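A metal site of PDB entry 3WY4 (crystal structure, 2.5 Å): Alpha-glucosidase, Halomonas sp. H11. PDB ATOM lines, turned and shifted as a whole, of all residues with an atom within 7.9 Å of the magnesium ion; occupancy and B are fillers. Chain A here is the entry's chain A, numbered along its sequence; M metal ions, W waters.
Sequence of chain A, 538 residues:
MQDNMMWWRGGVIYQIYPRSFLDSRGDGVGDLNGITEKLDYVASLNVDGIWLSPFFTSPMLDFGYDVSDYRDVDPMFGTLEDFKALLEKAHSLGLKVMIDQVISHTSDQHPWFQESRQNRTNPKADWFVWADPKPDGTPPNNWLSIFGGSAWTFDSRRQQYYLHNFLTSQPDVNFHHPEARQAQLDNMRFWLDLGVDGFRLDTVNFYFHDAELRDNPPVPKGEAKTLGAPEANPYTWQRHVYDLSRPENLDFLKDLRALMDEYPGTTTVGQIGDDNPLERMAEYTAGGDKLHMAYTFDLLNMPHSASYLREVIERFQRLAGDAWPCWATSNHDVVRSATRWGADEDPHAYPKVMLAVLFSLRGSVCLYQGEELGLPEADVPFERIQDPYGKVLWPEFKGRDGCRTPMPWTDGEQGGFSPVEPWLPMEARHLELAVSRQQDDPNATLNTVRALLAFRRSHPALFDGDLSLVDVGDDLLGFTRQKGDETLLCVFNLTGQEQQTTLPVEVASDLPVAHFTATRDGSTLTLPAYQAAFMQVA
OD1 of Asp 23 sits close to N of Arg 25, 3.0 Å away.
The backbone NH (N) of Val 29 lies close to the side-chain carboxylate (OD1) of Asp 27 (3.4 Å).
The side-chain carboxylate (OD2) of Asp 23 is in hydrogen-bond range of the backbone NH (N) of Gly 28, 3.0 Å away.
The backbone NH (N) of Asp 23 lies within hydrogen-bond range of the backbone carbonyl oxygen (O) of Phe 417 (3.1 Å).
The backbone NH (N) of Asp 31 is in hydrogen-bond range of the backbone carbonyl oxygen (O) of Leu 22 (3.1 Å).
The side-chain carboxylate of Asp 23 lies within hydrogen-bond range of the backbone NH of Gly 26 (3.2 Å).
The backbone NH of Asp 27 sits at hydrogen-bond distance from the side-chain carboxylate of Asp 23, 3.1 Å away.
OD1 of Asp 31 is in hydrogen-bond range of N of Asn 33.
Merely in contact with the magnesium ion: Arg 25 (3.8 Å) and Gly 30 (3.9 Å).
The magnesium ion is bound by O of Val 29 (2.1 Å).
Water W1 binds the magnesium ion (2.1 Å).
OD1 of Asp 23 is bound to the magnesium ion.
OD2 of Asp 31 binds the magnesium ion (2.4 Å).
The magnesium ion has four donor atoms within binding distance.
Slightly farther from the magnesium ion lies OD1 of Asp 27 (2.6 Å).
Water W1 bridges the side-chain carboxylate of Asp 27 (2.7 Å) and the backbone carbonyl oxygen of Met 76 (2.8 Å).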
ATOM      1  N   PRO A  18      -0.811 -33.002  21.029  1.00  0.00           N
ATOM      2  CA  PRO A  18      -1.084 -31.891  20.115  1.00  0.00           C
ATOM      3  C   PRO A  18      -0.263 -30.634  20.378  1.00  0.00           C
ATOM      4  O   PRO A  18       0.071 -29.916  19.439  1.00  0.00           O
ATOM      5  CB  PRO A  18      -2.563 -31.598  20.360  1.00  0.00           C
ATOM      6  CG  PRO A  18      -3.119 -32.889  20.822  1.00  0.00           C
ATOM      7  CD  PRO A  18      -2.039 -33.515  21.647  1.00  0.00           C
ATOM      8  N   ARG A  19       0.060 -30.373  21.641  1.00  0.00           N
ATOM      9  CA  ARG A  19       0.760 -29.153  22.016  1.00  0.00           C
ATOM     10  C   ARG A  19       2.242 -29.193  21.668  1.00  0.00           C
ATOM     11  O   ARG A  19       2.912 -28.159  21.672  1.00  0.00           O
ATOM     12  CB  ARG A  19       0.587 -28.888  23.505  1.00  0.00           C
ATOM     13  CG  ARG A  19      -0.580 -29.632  24.135  1.00  0.00           C
ATOM     14  CD  ARG A  19      -0.684 -29.342  25.624  1.00  0.00           C
ATOM     15  NE  ARG A  19      -1.744 -28.390  25.926  1.00  0.00           N
ATOM     16  CZ  ARG A  19      -1.600 -27.072  25.882  1.00  0.00           C
ATOM     17  NH1 ARG A  19      -0.444 -26.531  25.529  1.00  0.00           N
ATOM     18  NH2 ARG A  19      -2.624 -26.297  26.177  1.00  0.00           N
ATOM     19  N   LEU A  22       3.580 -30.197  16.225  1.00  0.00           N
ATOM     20  CA  LEU A  22       3.999 -29.209  15.239  1.00  0.00           C
ATOM     21  C   LEU A  22       3.169 -27.919  15.315  1.00  0.00           C
ATOM     22  O   LEU A  22       1.943 -27.954  15.261  1.00  0.00           O
ATOM     23  CB  LEU A  22       3.929 -29.777  13.825  1.00  0.00           C
ATOM     24  CG  LEU A  22       4.421 -28.833  12.717  1.00  0.00           C
ATOM     25  CD1 LEU A  22       5.897 -28.511  12.904  1.00  0.00           C
ATOM     26  CD2 LEU A  22       4.163 -29.414  11.338  1.00  0.00           C
ATOM     27  N   ASP A  23       3.865 -26.793  15.443  1.00  0.00           N
ATOM     28  CA  ASP A  23       3.228 -25.483  15.411  1.00  0.00           C
ATOM     29  C   ASP A  23       3.282 -24.923  13.994  1.00  0.00           C
ATOM     30  O   ASP A  23       4.366 -24.679  13.454  1.00  0.00           O
ATOM     31  CB  ASP A  23       3.912 -24.521  16.382  1.00  0.00           C
ATOM     32  CG  ASP A  23       3.441 -23.094  16.221  1.00  0.00           C
ATOM     33  OD1 ASP A  23       2.238 -22.877  15.956  1.00  0.00           O
ATOM     34  OD2 ASP A  23       4.275 -22.176  16.345  1.00  0.00           O
ATOM     35  N   SER A  24       2.115 -24.714  13.392  1.00  0.00           N
ATOM     36  CA  SER A  24       2.044 -24.205  12.024  1.00  0.00           C
ATOM     37  C   SER A  24       1.492 -22.784  11.982  1.00  0.00           C
ATOM     38  O   SER A  24       1.300 -22.218  10.909  1.00  0.00           O
ATOM     39  CB  SER A  24       1.176 -25.129  11.169  1.00  0.00           C
ATOM     40  OG  SER A  24      -0.164 -25.150  11.620  1.00  0.00           O
ATOM     41  N   ARG A  25       1.234 -22.225  13.164  1.00  0.00           N
ATOM     42  CA  ARG A  25       0.615 -20.902  13.258  1.00  0.00           C
ATOM     43  C   ARG A  25       1.549 -19.850  13.847  1.00  0.00           C
ATOM     44  O   ARG A  25       1.214 -18.665  13.913  1.00  0.00           O
ATOM     45  CB  ARG A  25      -0.677 -20.981  14.060  1.00  0.00           C
ATOM     46  CG  ARG A  25      -1.690 -21.982  13.522  1.00  0.00           C
ATOM     47  CD  ARG A  25      -1.886 -21.825  12.018  1.00  0.00           C
ATOM     48  NE  ARG A  25      -2.848 -22.794  11.501  1.00  0.00           N
ATOM     49  CZ  ARG A  25      -4.098 -22.507  11.168  1.00  0.00           C
ATOM     50  NH1 ARG A  25      -4.549 -21.271  11.316  1.00  0.00           N
ATOM     51  NH2 ARG A  25      -4.897 -23.442  10.701  1.00  0.00           N
ATOM     52  N   GLY A  26       2.732 -20.294  14.277  1.00  0.00           N
ATOM     53  CA  GLY A  26       3.747 -19.388  14.789  1.00  0.00           C
ATOM     54  C   GLY A  26       3.405 -18.734  16.110  1.00  0.00           C
ATOM     55  O   GLY A  26       3.704 -17.555  16.325  1.00  0.00           O
ATOM     56  N   ASP A  27       2.789 -19.490  17.009  1.00  0.00           N
ATOM     57  CA  ASP A  27       2.485 -18.982  18.348  1.00  0.00           C
ATOM     58  C   ASP A  27       3.200 -19.786  19.430  1.00  0.00           C
ATOM     59  O   ASP A  27       3.036 -19.526  20.627  1.00  0.00           O
ATOM     60  CB  ASP A  27       0.967 -18.953  18.600  1.00  0.00           C
ATOM     61  CG  ASP A  27       0.319 -20.314  18.441  1.00  0.00           C
ATOM     62  OD1 ASP A  27       0.966 -21.217  17.871  1.00  0.00           O
ATOM     63  OD2 ASP A  27      -0.838 -20.472  18.864  1.00  0.00           O
ATOM     64  N   GLY A  28       3.992 -20.768  19.014  1.00  0.00           N
ATOM     65  CA  GLY A  28       4.794 -21.555  19.931  1.00  0.00           C
ATOM     66  C   GLY A  28       4.098 -22.800  20.433  1.00  0.00           C
ATOM     67  O   GLY A  28       4.713 -23.641  21.091  1.00  0.00           O
ATOM     68  N   VAL A  29       2.807 -22.931  20.137  1.00  0.00           N
ATOM     69  CA  VAL A  29       2.033 -24.080  20.571  1.00  0.00           C
ATOM     70  C   VAL A  29       1.608 -24.922  19.372  1.00  0.00           C
ATOM     71  O   VAL A  29       1.180 -24.391  18.346  1.00  0.00           O
ATOM     72  CB  VAL A  29       0.779 -23.654  21.358  1.00  0.00           C
ATOM     73  CG1 VAL A  29       0.012 -24.867  21.855  1.00  0.00           C
ATOM     74  CG2 VAL A  29       1.169 -22.759  22.527  1.00  0.00           C
ATOM     75  N   GLY A  30       1.752 -26.240  19.503  1.00  0.00           N
ATOM     76  CA  GLY A  30       1.340 -27.147  18.444  1.00  0.00           C
ATOM     77  C   GLY A  30      -0.156 -27.078  18.192  1.00  0.00           C
ATOM     78  O   GLY A  30      -0.935 -26.782  19.093  1.00  0.00           O
ATOM     79  N   ASP A  31      -0.549 -27.334  16.941  1.00  0.00           N
ATOM     80  CA  ASP A  31      -1.963 -27.279  16.563  1.00  0.00           C
ATOM     81  C   ASP A  31      -2.342 -28.454  15.670  1.00  0.00           C
ATOM     82  O   ASP A  31      -1.494 -29.266  15.298  1.00  0.00           O
ATOM     83  CB  ASP A  31      -2.269 -25.950  15.873  1.00  0.00           C
ATOM     84  CG  ASP A  31      -1.300 -25.639  14.750  1.00  0.00           C
ATOM     85  OD1 ASP A  31      -1.535 -26.111  13.616  1.00  0.00           O
ATOM     86  OD2 ASP A  31      -0.318 -24.915  14.997  1.00  0.00           O
ATOM     87  N   LEU A  32      -3.628 -28.539  15.333  1.00  0.00           N
ATOM     88  CA  LEU A  32      -4.159 -29.666  14.574  1.00  0.00           C
ATOM     89  C   LEU A  32      -3.620 -29.724  13.139  1.00  0.00           C
ATOM     90  O   LEU A  32      -3.312 -30.801  12.631  1.00  0.00           O
ATOM     91  CB  LEU A  32      -5.688 -29.641  14.549  1.00  0.00           C
ATOM     92  CG  LEU A  32      -6.385 -29.776  15.907  1.00  0.00           C
ATOM     93  CD1 LEU A  32      -7.891 -29.843  15.726  1.00  0.00           C
ATOM     94  CD2 LEU A  32      -5.879 -30.983  16.664  1.00  0.00           C
ATOM     95  N   ASN A  33      -3.503 -28.570  12.493  1.00  0.00           N
ATOM     96  CA  ASN A  33      -3.035 -28.512  11.110  1.00  0.00           C
ATOM     97  C   ASN A  33      -1.584 -28.956  10.952  1.00  0.00           C
ATOM     98  O   ASN A  33      -1.191 -29.420   9.887  1.00  0.00           O
ATOM     99  CB  ASN A  33      -3.246 -27.112  10.520  1.00  0.00           C
ATOM    100  CG  ASN A  33      -4.712 -26.808  10.265  1.00  0.00           C
ATOM    101  OD1 ASN A  33      -5.141 -25.658  10.390  1.00  0.00           O
ATOM    102  ND2 ASN A  33      -5.478 -27.829   9.917  1.00  0.00           N
ATOM    103  N   GLY A  34      -0.799 -28.820  12.010  1.00  0.00           N
ATOM    104  CA  GLY A  34       0.566 -29.316  12.013  1.00  0.00           C
ATOM    105  C   GLY A  34       0.587 -30.830  12.007  1.00  0.00           C
ATOM    106  O   GLY A  34       1.351 -31.461  11.260  1.00  0.00           O
ATOM    107  N   PRO A  75      -9.699 -23.125  20.403  1.00  0.00           N
ATOM    108  CA  PRO A  75      -9.189 -22.208  19.375  1.00  0.00           C
ATOM    109  C   PRO A  75      -7.672 -22.173  19.281  1.00  0.00           C
ATOM    110  O   PRO A  75      -7.133 -21.730  18.261  1.00  0.00           O
ATOM    111  CB  PRO A  75      -9.735 -20.842  19.809  1.00  0.00           C
ATOM    112  CG  PRO A  75     -10.155 -21.014  21.236  1.00  0.00           C
ATOM    113  CD  PRO A  75     -10.601 -22.433  21.346  1.00  0.00           C
ATOM    114  N   MET A  76      -6.986 -22.619  20.323  1.00  0.00           N
ATOM    115  CA  MET A  76      -5.528 -22.648  20.339  1.00  0.00           C
ATOM    116  C   MET A  76      -4.994 -23.784  19.471  1.00  0.00           C
ATOM    117  O   MET A  76      -3.881 -23.708  18.945  1.00  0.00           O
ATOM    118  CB  MET A  76      -5.016 -22.789  21.769  1.00  0.00           C
ATOM    119  CG  MET A  76      -3.529 -22.569  21.923  1.00  0.00           C
ATOM    120  SD  MET A  76      -2.947 -23.169  23.514  1.00  0.00           S
ATOM    121  CE  MET A  76      -3.554 -24.852  23.461  1.00  0.00           C
ATOM    122  N   PHE A  77      -5.795 -24.838  19.321  1.00  0.00           N
ATOM    123  CA  PHE A  77      -5.406 -25.982  18.514  1.00  0.00           C
ATOM    124  C   PHE A  77      -5.975 -25.892  17.100  1.00  0.00           C
ATOM    125  O   PHE A  77      -5.465 -26.523  16.171  1.00  0.00           O
ATOM    126  CB  PHE A  77      -5.846 -27.285  19.176  1.00  0.00           C
ATOM    127  CG  PHE A  77      -5.050 -27.646  20.394  1.00  0.00           C
ATOM    128  CD1 PHE A  77      -3.657 -27.610  20.380  1.00  0.00           C
ATOM    129  CD2 PHE A  77      -5.681 -28.008  21.570  1.00  0.00           C
ATOM    130  CE1 PHE A  77      -2.929 -27.933  21.507  1.00  0.00           C
ATOM    131  CE2 PHE A  77      -4.963 -28.345  22.699  1.00  0.00           C
ATOM    132  CZ  PHE A  77      -3.582 -28.304  22.663  1.00  0.00           C
ATOM    133  N   GLY A  78      -7.050 -25.125  16.951  1.00  0.00           N
ATOM    134  CA  GLY A  78      -7.694 -24.963  15.656  1.00  0.00           C
ATOM    135  C   GLY A  78      -9.202 -24.977  15.740  1.00  0.00           C
ATOM    136  O   GLY A  78      -9.785 -24.475  16.701  1.00  0.00           O
ATOM    137  N   PHE A 417      10.182 -26.877  14.907  1.00  0.00           N
ATOM    138  CA  PHE A 417       8.867 -27.063  15.493  1.00  0.00           C
ATOM    139  C   PHE A 417       8.058 -25.770  15.439  1.00  0.00           C
ATOM    140  O   PHE A 417       6.832 -25.795  15.263  1.00  0.00           O
ATOM    141  CB  PHE A 417       8.993 -27.534  16.939  1.00  0.00           C
ATOM    142  CG  PHE A 417       7.722 -27.420  17.743  1.00  0.00           C
ATOM    143  CD1 PHE A 417       6.730 -28.388  17.634  1.00  0.00           C
ATOM    144  CD2 PHE A 417       7.510 -26.350  18.587  1.00  0.00           C
ATOM    145  CE1 PHE A 417       5.565 -28.282  18.367  1.00  0.00           C
ATOM    146  CE2 PHE A 417       6.345 -26.237  19.326  1.00  0.00           C
ATOM    147  CZ  PHE A 417       5.373 -27.211  19.210  1.00  0.00           C
ATOM    148  N   SER A 418       8.735 -24.636  15.589  1.00  0.00           N
ATOM    149  CA  SER A 418       8.084 -23.348  15.631  1.00  0.00           C
ATOM    150  C   SER A 418       9.056 -22.226  15.271  1.00  0.00           C
ATOM    151  O   SER A 418      10.238 -22.301  15.616  1.00  0.00           O
ATOM    152  CB  SER A 418       7.483 -23.105  17.017  1.00  0.00           C
ATOM    153  OG  SER A 418       6.805 -21.859  17.079  1.00  0.00           O
HETATM  154 MG    MG M   1       0.127 -23.459  16.820  1.00  0.00          MG
HETATM  155  O   HOH W   1      -1.735 -22.627  17.475  1.00  0.00           O
